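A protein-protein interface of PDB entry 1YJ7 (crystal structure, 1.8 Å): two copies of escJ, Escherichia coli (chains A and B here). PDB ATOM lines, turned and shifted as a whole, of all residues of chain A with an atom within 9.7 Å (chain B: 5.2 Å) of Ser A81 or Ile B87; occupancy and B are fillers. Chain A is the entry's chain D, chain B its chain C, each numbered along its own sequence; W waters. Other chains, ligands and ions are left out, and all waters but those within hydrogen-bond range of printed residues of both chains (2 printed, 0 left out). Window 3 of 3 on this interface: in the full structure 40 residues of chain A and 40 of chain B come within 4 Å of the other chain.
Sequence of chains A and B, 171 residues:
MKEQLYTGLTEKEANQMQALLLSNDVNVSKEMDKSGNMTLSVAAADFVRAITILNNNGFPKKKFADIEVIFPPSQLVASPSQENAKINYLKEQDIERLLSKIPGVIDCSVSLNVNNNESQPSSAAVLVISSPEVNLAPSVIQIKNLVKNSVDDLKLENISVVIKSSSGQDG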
ATOM      1  N   ALA A  65     -17.158   5.318   7.682  1.00  0.00           N
ATOM      2  CA  ALA A  65     -16.101   4.561   8.365  1.00  0.00           C
ATOM      3  C   ALA A  65     -16.603   3.209   8.843  1.00  0.00           C
ATOM      4  O   ALA A  65     -17.721   3.075   9.355  1.00  0.00           O
ATOM      5  CB  ALA A  65     -15.538   5.347   9.528  1.00  0.00           C
ATOM      6  N   ILE A  67     -16.036   0.177  11.393  1.00  0.00           N
ATOM      7  CA  ILE A  67     -15.435  -0.073  12.706  1.00  0.00           C
ATOM      8  C   ILE A  67     -14.256  -1.052  12.626  1.00  0.00           C
ATOM      9  O   ILE A  67     -13.308  -0.935  13.384  1.00  0.00           O
ATOM     10  CB  ILE A  67     -16.502  -0.583  13.704  1.00  0.00           C
ATOM     11  CG1 ILE A  67     -15.933  -0.666  15.117  1.00  0.00           C
ATOM     12  CG2 ILE A  67     -17.111  -1.917  13.253  1.00  0.00           C
ATOM     13  CD1 ILE A  67     -17.026  -0.839  16.175  1.00  0.00           C
ATOM     14  N   ILE A  70     -11.215   1.147  11.479  1.00  0.00           N
ATOM     15  CA  ILE A  70     -10.778   2.031  12.567  1.00  0.00           C
ATOM     16  C   ILE A  70     -10.122   1.239  13.712  1.00  0.00           C
ATOM     17  O   ILE A  70      -9.136   1.690  14.289  1.00  0.00           O
ATOM     18  CB  ILE A  70     -11.970   2.881  13.110  1.00  0.00           C
ATOM     19  CG1 ILE A  70     -12.587   3.753  12.004  1.00  0.00           C
ATOM     20  CG2 ILE A  70     -11.535   3.756  14.290  1.00  0.00           C
ATOM     21  CD1 ILE A  70     -11.564   4.488  11.129  1.00  0.00           C
ATOM     22  N   PHE A  71     -10.670   0.061  14.015  1.00  0.00           N
ATOM     23  CA  PHE A  71     -10.174  -0.808  15.087  1.00  0.00           C
ATOM     24  C   PHE A  71      -9.970  -2.233  14.539  1.00  0.00           C
ATOM     25  O   PHE A  71     -10.787  -3.120  14.798  1.00  0.00           O
ATOM     26  CB  PHE A  71     -11.174  -0.859  16.247  1.00  0.00           C
ATOM     27  CG  PHE A  71     -11.414   0.459  16.931  1.00  0.00           C
ATOM     28  CD1 PHE A  71     -12.707   0.949  17.082  1.00  0.00           C
ATOM     29  CD2 PHE A  71     -10.357   1.196  17.454  1.00  0.00           C
ATOM     30  CE1 PHE A  71     -12.940   2.151  17.722  1.00  0.00           C
ATOM     31  CE2 PHE A  71     -10.583   2.402  18.092  1.00  0.00           C
ATOM     32  CZ  PHE A  71     -11.873   2.884  18.227  1.00  0.00           C
ATOM     33  N   SER A  79      -8.368  -3.595  24.171  1.00  0.00           N
ATOM     34  CA  SER A  79      -8.630  -2.382  24.946  1.00  0.00           C
ATOM     35  C   SER A  79     -10.094  -2.363  25.395  1.00  0.00           C
ATOM     36  O   SER A  79     -10.972  -2.678  24.594  1.00  0.00           O
ATOM     37  CB  SER A  79      -8.301  -1.139  24.099  1.00  0.00           C
ATOM     38  OG  SER A  79      -9.189  -0.053  24.346  1.00  0.00           O
ATOM     39  N   PRO A  80     -10.365  -2.013  26.657  1.00  0.00           N
ATOM     40  CA  PRO A  80     -11.744  -1.912  27.159  1.00  0.00           C
ATOM     41  C   PRO A  80     -12.703  -1.065  26.309  1.00  0.00           C
ATOM     42  O   PRO A  80     -13.804  -1.518  26.006  1.00  0.00           O
ATOM     43  CB  PRO A  80     -11.570  -1.273  28.541  1.00  0.00           C
ATOM     44  CG  PRO A  80     -10.195  -1.686  28.975  1.00  0.00           C
ATOM     45  CD  PRO A  80      -9.377  -1.753  27.722  1.00  0.00           C
ATOM     46  N   SER A  81     -12.304   0.147  25.948  1.00  0.00           N
ATOM     47  CA  SER A  81     -13.195   1.042  25.203  1.00  0.00           C
ATOM     48  C   SER A  81     -13.404   0.575  23.764  1.00  0.00           C
ATOM     49  O   SER A  81     -14.474   0.777  23.198  1.00  0.00           O
ATOM     50  CB  SER A  81     -12.639   2.462  25.202  1.00  0.00           C
ATOM     51  OG  SER A  81     -11.492   2.513  24.389  1.00  0.00           O
ATOM     52  N   GLN A  82     -12.375  -0.030  23.182  1.00  0.00           N
ATOM     53  CA  GLN A  82     -12.442  -0.585  21.833  1.00  0.00           C
ATOM     54  C   GLN A  82     -13.368  -1.813  21.805  1.00  0.00           C
ATOM     55  O   GLN A  82     -14.187  -1.983  20.897  1.00  0.00           O
ATOM     56  CB  GLN A  82     -11.049  -0.981  21.366  1.00  0.00           C
ATOM     57  CG  GLN A  82     -11.005  -1.632  20.003  1.00  0.00           C
ATOM     58  CD  GLN A  82      -9.599  -1.896  19.510  1.00  0.00           C
ATOM     59  OE1 GLN A  82      -8.720  -1.032  19.611  1.00  0.00           O
ATOM     60  NE2 GLN A  82      -9.380  -3.089  18.960  1.00  0.00           N
ATOM     61  N   GLU A  83     -13.217  -2.665  22.812  1.00  0.00           N
ATOM     62  CA  GLU A  83     -14.062  -3.844  22.959  1.00  0.00           C
ATOM     63  C   GLU A  83     -15.520  -3.466  23.070  1.00  0.00           C
ATOM     64  O   GLU A  83     -16.380  -4.074  22.436  1.00  0.00           O
ATOM     65  CB  GLU A  83     -13.668  -4.597  24.233  1.00  0.00           C
ATOM     66  CG  GLU A  83     -14.532  -5.804  24.528  1.00  0.00           C
ATOM     67  CD  GLU A  83     -14.473  -6.820  23.415  1.00  0.00           C
ATOM     68  OE1 GLU A  83     -13.493  -6.780  22.637  1.00  0.00           O
ATOM     69  OE2 GLU A  83     -15.404  -7.661  23.325  1.00  0.00           O
ATOM     70  N   ASN A  84     -15.787  -2.479  23.909  1.00  0.00           N
ATOM     71  CA  ASN A  84     -17.133  -2.020  24.156  1.00  0.00           C
ATOM     72  C   ASN A  84     -17.759  -1.406  22.897  1.00  0.00           C
ATOM     73  O   ASN A  84     -18.958  -1.522  22.699  1.00  0.00           O
ATOM     74  CB  ASN A  84     -17.164  -1.005  25.288  1.00  0.00           C
ATOM     75  CG  ASN A  84     -16.886  -1.638  26.662  1.00  0.00           C
ATOM     76  OD1 ASN A  84     -16.918  -0.940  27.695  1.00  0.00           O
ATOM     77  ND2 ASN A  84     -16.597  -2.946  26.680  1.00  0.00           N
ATOM     78  N   ALA A  85     -16.949  -0.752  22.061  1.00  0.00           N
ATOM     79  CA  ALA A  85     -17.474  -0.190  20.802  1.00  0.00           C
ATOM     80  C   ALA A  85     -17.891  -1.319  19.872  1.00  0.00           C
ATOM     81  O   ALA A  85     -18.881  -1.197  19.156  1.00  0.00           O
ATOM     82  CB  ALA A  85     -16.436   0.688  20.115  1.00  0.00           C
ATOM     83  N   LYS A  86     -17.131  -2.416  19.889  1.00  0.00           N
ATOM     84  CA  LYS A  86     -17.436  -3.574  19.062  1.00  0.00           C
ATOM     85  C   LYS A  86     -18.680  -4.302  19.580  1.00  0.00           C
ATOM     86  O   LYS A  86     -19.512  -4.737  18.789  1.00  0.00           O
ATOM     87  CB  LYS A  86     -16.223  -4.511  18.942  1.00  0.00           C
ATOM     88  CG  LYS A  86     -15.209  -3.988  17.924  1.00  0.00           C
ATOM     89  CD  LYS A  86     -14.014  -4.882  17.744  1.00  0.00           C
ATOM     90  CE  LYS A  86     -12.971  -4.189  16.878  1.00  0.00           C
ATOM     91  NZ  LYS A  86     -11.931  -5.114  16.334  1.00  0.00           N
ATOM     92  N   ILE A  87     -18.813  -4.406  20.902  1.00  0.00           N
ATOM     93  CA  ILE A  87     -20.011  -4.983  21.517  1.00  0.00           C
ATOM     94  C   ILE A  87     -21.256  -4.140  21.188  1.00  0.00           C
ATOM     95  O   ILE A  87     -22.321  -4.680  20.898  1.00  0.00           O
ATOM     96  CB  ILE A  87     -19.821  -5.108  23.062  1.00  0.00           C
ATOM     97  CG1 ILE A  87     -18.797  -6.211  23.398  1.00  0.00           C
ATOM     98  CG2 ILE A  87     -21.147  -5.336  23.767  1.00  0.00           C
ATOM     99  CD1 ILE A  87     -19.268  -7.628  23.123  1.00  0.00           C
ATOM    100  N   ASN A  88     -21.122  -2.816  21.253  1.00  0.00           N
ATOM    101  CA  ASN A  88     -22.220  -1.911  20.925  1.00  0.00           C
ATOM    102  C   ASN A  88     -22.637  -2.061  19.474  1.00  0.00           C
ATOM    103  O   ASN A  88     -23.818  -2.053  19.163  1.00  0.00           O
ATOM    104  CB  ASN A  88     -21.780  -0.455  21.154  1.00  0.00           C
ATOM    105  CG  ASN A  88     -22.921   0.519  21.107  1.00  0.00           C
ATOM    106  OD1 ASN A  88     -23.815   0.473  21.958  1.00  0.00           O
ATOM    107  ND2 ASN A  88     -22.889   1.456  20.123  1.00  0.00           N
ATOM    108  N   TYR A  89     -21.651  -2.183  18.597  1.00  0.00           N
ATOM    109  CA  TYR A  89     -21.889  -2.310  17.161  1.00  0.00           C
ATOM    110  C   TYR A  89     -22.607  -3.613  16.857  1.00  0.00           C
ATOM    111  O   TYR A  89     -23.584  -3.642  16.095  1.00  0.00           O
ATOM    112  CB  TYR A  89     -20.556  -2.235  16.420  1.00  0.00           C
ATOM    113  CG  TYR A  89     -20.606  -2.617  14.966  1.00  0.00           C
ATOM    114  CD1 TYR A  89     -21.167  -1.757  14.014  1.00  0.00           C
ATOM    115  CD2 TYR A  89     -20.073  -3.818  14.528  1.00  0.00           C
ATOM    116  CE1 TYR A  89     -21.205  -2.101  12.673  1.00  0.00           C
ATOM    117  CE2 TYR A  89     -20.091  -4.164  13.186  1.00  0.00           C
ATOM    118  CZ  TYR A  89     -20.663  -3.300  12.270  1.00  0.00           C
ATOM    119  OH  TYR A  89     -20.685  -3.641  10.934  1.00  0.00           O
ATOM    120  N   SER A 111     -28.566   3.579  16.186  1.00  0.00           N
ATOM    121  CA  SER A 111     -27.392   4.072  16.881  1.00  0.00           C
ATOM    122  C   SER A 111     -27.685   4.040  18.375  1.00  0.00           C
ATOM    123  O   SER A 111     -28.642   4.685  18.833  1.00  0.00           O
ATOM    124  CB  SER A 111     -27.029   5.494  16.434  1.00  0.00           C
ATOM    125  OG  SER A 111     -25.843   5.925  17.091  1.00  0.00           O
ATOM    126  N   LEU A 112     -26.879   3.274  19.116  1.00  0.00           N
ATOM    127  CA  LEU A 112     -27.037   3.090  20.556  1.00  0.00           C
ATOM    128  C   LEU A 112     -26.037   3.897  21.373  1.00  0.00           C
ATOM    129  O   LEU A 112     -24.862   3.954  21.030  1.00  0.00           O
ATOM    130  CB  LEU A 112     -26.832   1.628  20.938  1.00  0.00           C
ATOM    131  CG  LEU A 112     -27.861   0.644  20.421  1.00  0.00           C
ATOM    132  CD1 LEU A 112     -27.436  -0.745  20.858  1.00  0.00           C
ATOM    133  CD2 LEU A 112     -29.277   0.964  20.906  1.00  0.00           C
ATOM    134  N   VAL A 114     -25.026   3.414  25.109  1.00  0.00           N
ATOM    135  CA  VAL A 114     -25.079   2.582  26.314  1.00  0.00           C
ATOM    136  C   VAL A 114     -23.920   2.959  27.243  1.00  0.00           C
ATOM    137  O   VAL A 114     -22.761   2.847  26.826  1.00  0.00           O
ATOM    138  CB  VAL A 114     -24.967   1.106  25.947  1.00  0.00           C
ATOM    139  CG1 VAL A 114     -24.901   0.228  27.207  1.00  0.00           C
ATOM    140  CG2 VAL A 114     -26.111   0.722  25.085  1.00  0.00           C
ATOM    141  N   GLU B  83      -7.540   7.230  21.586  1.00  0.00           N
ATOM    142  CA  GLU B  83      -8.580   6.214  21.567  1.00  0.00           C
ATOM    143  C   GLU B  83      -9.927   6.889  21.524  1.00  0.00           C
ATOM    144  O   GLU B  83     -10.788   6.516  20.728  1.00  0.00           O
ATOM    145  CB  GLU B  83      -8.476   5.357  22.833  1.00  0.00           C
ATOM    146  CG  GLU B  83      -9.436   4.187  22.887  1.00  0.00           C
ATOM    147  CD  GLU B  83      -8.880   2.974  22.176  1.00  0.00           C
ATOM    148  OE1 GLU B  83      -8.404   2.034  22.869  1.00  0.00           O
ATOM    149  OE2 GLU B  83      -8.908   2.977  20.924  1.00  0.00           O
ATOM    150  N   ASN B  84     -10.105   7.883  22.386  1.00  0.00           N
ATOM    151  CA  ASN B  84     -11.369   8.586  22.495  1.00  0.00           C
ATOM    152  C   ASN B  84     -11.670   9.418  21.252  1.00  0.00           C
ATOM    153  O   ASN B  84     -12.829   9.608  20.919  1.00  0.00           O
ATOM    154  CB  ASN B  84     -11.408   9.479  23.734  1.00  0.00           C
ATOM    155  CG  ASN B  84     -11.265   8.687  25.046  1.00  0.00           C
ATOM    156  OD1 ASN B  84     -10.852   9.244  26.071  1.00  0.00           O
ATOM    157  ND2 ASN B  84     -11.599   7.394  25.013  1.00  0.00           N
ATOM    158  N   ALA B  85     -10.632   9.935  20.595  1.00  0.00           N
ATOM    159  CA  ALA B  85     -10.815  10.634  19.315  1.00  0.00           C
ATOM    160  C   ALA B  85     -11.374   9.682  18.269  1.00  0.00           C
ATOM    161  O   ALA B  85     -12.243  10.056  17.473  1.00  0.00           O
ATOM    162  CB  ALA B  85      -9.500  11.210  18.823  1.00  0.00           C
ATOM    163  N   LYS B  86     -10.870   8.450  18.278  1.00  0.00           N
ATOM    164  CA  LYS B  86     -11.304   7.438  17.327  1.00  0.00           C
ATOM    165  C   LYS B  86     -12.723   6.943  17.624  1.00  0.00           C
ATOM    166  O   LYS B  86     -13.488   6.714  16.703  1.00  0.00           O
ATOM    167  CB  LYS B  86     -10.303   6.275  17.244  1.00  0.00           C
ATOM    168  CG  LYS B  86      -9.050   6.643  16.427  1.00  0.00           C
ATOM    169  CD  LYS B  86      -8.108   5.470  16.163  1.00  0.00           C
ATOM    170  CE  LYS B  86      -6.834   5.971  15.463  1.00  0.00           C
ATOM    171  NZ  LYS B  86      -5.766   4.931  15.274  1.00  0.00           N
ATOM    172  N   ILE B  87     -13.066   6.813  18.898  1.00  0.00           N
ATOM    173  CA  ILE B  87     -14.420   6.460  19.319  1.00  0.00           C
ATOM    174  C   ILE B  87     -15.420   7.566  18.933  1.00  0.00           C
ATOM    175  O   ILE B  87     -16.530   7.289  18.497  1.00  0.00           O
ATOM    176  CB  ILE B  87     -14.454   6.217  20.859  1.00  0.00           C
ATOM    177  CG1 ILE B  87     -13.676   4.945  21.228  1.00  0.00           C
ATOM    178  CG2 ILE B  87     -15.880   6.194  21.389  1.00  0.00           C
ATOM    179  CD1 ILE B  87     -14.440   3.657  21.003  1.00  0.00           C
ATOM    180  N   ASN B  88     -15.026   8.816  19.121  1.00  0.00           N
ATOM    181  CA  ASN B  88     -15.850   9.960  18.730  1.00  0.00           C
ATOM    182  C   ASN B  88     -16.056   9.997  17.213  1.00  0.00           C
ATOM    183  O   ASN B  88     -17.144  10.259  16.734  1.00  0.00           O
ATOM    184  CB  ASN B  88     -15.158  11.253  19.172  1.00  0.00           C
ATOM    185  CG  ASN B  88     -16.034  12.471  19.043  1.00  0.00           C
ATOM    186  OD1 ASN B  88     -17.043  12.582  19.739  1.00  0.00           O
ATOM    187  ND2 ASN B  88     -15.623  13.435  18.194  1.00  0.00           N
ATOM    188  N   TYR B  89     -14.997   9.750  16.472  1.00  0.00           N
ATOM    189  CA  TYR B  89     -15.069   9.727  15.017  1.00  0.00           C
ATOM    190  C   TYR B  89     -16.014   8.626  14.541  1.00  0.00           C
ATOM    191  O   TYR B  89     -16.842   8.844  13.653  1.00  0.00           O
ATOM    192  CB  TYR B  89     -13.684   9.526  14.432  1.00  0.00           C
ATOM    193  CG  TYR B  89     -13.647   9.298  12.954  1.00  0.00           C
ATOM    194  CD1 TYR B  89     -13.906  10.337  12.058  1.00  0.00           C
ATOM    195  CD2 TYR B  89     -13.330   8.058  12.435  1.00  0.00           C
ATOM    196  CE1 TYR B  89     -13.862  10.131  10.708  1.00  0.00           C
ATOM    197  CE2 TYR B  89     -13.281   7.847  11.081  1.00  0.00           C
ATOM    198  CZ  TYR B  89     -13.533   8.887  10.219  1.00  0.00           C
ATOM    199  OH  TYR B  89     -13.478   8.655   8.866  1.00  0.00           O
ATOM    200  N   LEU B  90     -15.906   7.448  15.149  1.00  0.00           N
ATOM    201  CA  LEU B  90     -16.834   6.360  14.812  1.00  0.00           C
ATOM    202  C   LEU B  90     -18.281   6.773  15.036  1.00  0.00           C
ATOM    203  O   LEU B  90     -19.140   6.482  14.203  1.00  0.00           O
ATOM    204  CB  LEU B  90     -16.492   5.091  15.592  1.00  0.00           C
ATOM    205  CG  LEU B  90     -17.447   3.899  15.455  1.00  0.00           C
ATOM    206  CD1 LEU B  90     -17.388   3.298  14.064  1.00  0.00           C
ATOM    207  CD2 LEU B  90     -17.120   2.869  16.514  1.00  0.00           C
ATOM    208  N   LYS B  91     -18.570   7.443  16.151  1.00  0.00           N
ATOM    209  CA  LYS B  91     -19.923   7.911  16.420  1.00  0.00           C
ATOM    210  C   LYS B  91     -20.371   8.939  15.395  1.00  0.00           C
ATOM    211  O   LYS B  91     -21.496   8.892  14.913  1.00  0.00           O
ATOM    212  CB  LYS B  91     -20.058   8.472  17.854  1.00  0.00           C
ATOM    213  CG  LYS B  91     -21.493   8.894  18.238  1.00  0.00           C
ATOM    214  CD  LYS B  91     -22.516   7.760  18.233  1.00  0.00           C
ATOM    215  CE  LYS B  91     -22.293   6.738  19.334  1.00  0.00           C
ATOM    216  NZ  LYS B  91     -23.497   5.808  19.470  1.00  0.00           N
HETATM  217  O   HOH W   1     -23.613   4.329  17.048  1.00  0.00           O
HETATM  218  O   HOH W   2     -21.999   4.986  21.914  1.00  0.00           O
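Printed residues of chain B within 4 Å of Ala A65: Tyr B89 (3.7 Å). Printed residues of chain B within 4 Å of Ile A70: Tyr B89 (3.8 Å). Ser A81 touches two residues of chain B. Of the printed residues of chain B, Ala A85 touches Ile B87. Printed residues of chain A within 4 Å of Tyr B89: Ala A65 (3.7 Å) and Ile A70 (3.8 Å). Printed residues of chain A within 4 Å of Leu B90: Ile A67. The nearest residue of chain B that does not touch Ser A81 is Asn B84 (4.9 Å). The nearest printed residue of chain B that does not touch Ala A85 is Leu B90 (4.3 Å).
O of Phe A71 sits at hydrogen-bond distance from NZ of Lys A86. The side-chain hydroxyl (OG) of Ser A79 is in hydrogen-bond range of the side-chain hydroxyl (OG) of Ser A81 (3.4 Å). The side-chain hydroxyl (OG) of Ser A79 lies within hydrogen-bond range of the backbone NH (N) of Gln A82 (3.4 Å). The side-chain amide nitrogen (ND2) of Asn A88 lies within hydrogen-bond range of the backbone carbonyl oxygen (O) of Leu A112, 3.3 Å away.
Ala A85 touches Ile B87, but with the chains exchanged Ile A87 does not touch Ala B85 (16.1 Å).
Of the 18 printed residues of chain A, 9 touch a printed residue of chain B. Printed residues of chain B that touch a printed residue of chain A: Glu B83, Lys B86, Ile B87, Tyr B89, Leu B90 and Lys B91. Hydrophobic or aromatic side chains of chain B that line the printed part of chain A: Ile B87, Tyr B89 and Leu B90. Along chain B the printed residues that touch a printed residue of chain A span positions 83 to 91. Among the printed residues, no Asp or Glu carboxylate lies within 4 Å of a Lys or Arg side-chain nitrogen of the other chain.
OE1 of Glu B83 is in hydrogen-bond range of OG of Ser A79, 2.7 Å away. OG of Ser A81 lies close to OE1 of Glu B83, 3.5 Å away. NZ of Lys B91 lies within hydrogen-bond range of OG of Ser A111, at 3.3 Å. NZ of Lys B91 sits at hydrogen-bond distance from O of Leu A112.
Water W1 bridges the side-chain hydroxyl (OG) of Ser A111 (2.7 Å) and the side-chain amino group (NZ) of Lys B91 (2.8 Å). Water W2 bridges NZ of Lys B91 (3.0 Å) and O of Leu A112 (3.2 Å).
Among the printed residues, pairs that only touch across the chains: Ala A65 with Tyr B89 (3.7 Å), Ile A67 with Leu B90 (3.7 Å), Ile A70 with Tyr B89 (3.8 Å), Phe A71 with Glu B83 (3.3 Å), Phe A71 with Lys B86 (3.9 Å), Phe A71 with Ile B87 (3.9 Å), Ser A81 with Ile B87 (3.6 Å) and Ala A85 with Ile B87 (3.7 Å).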
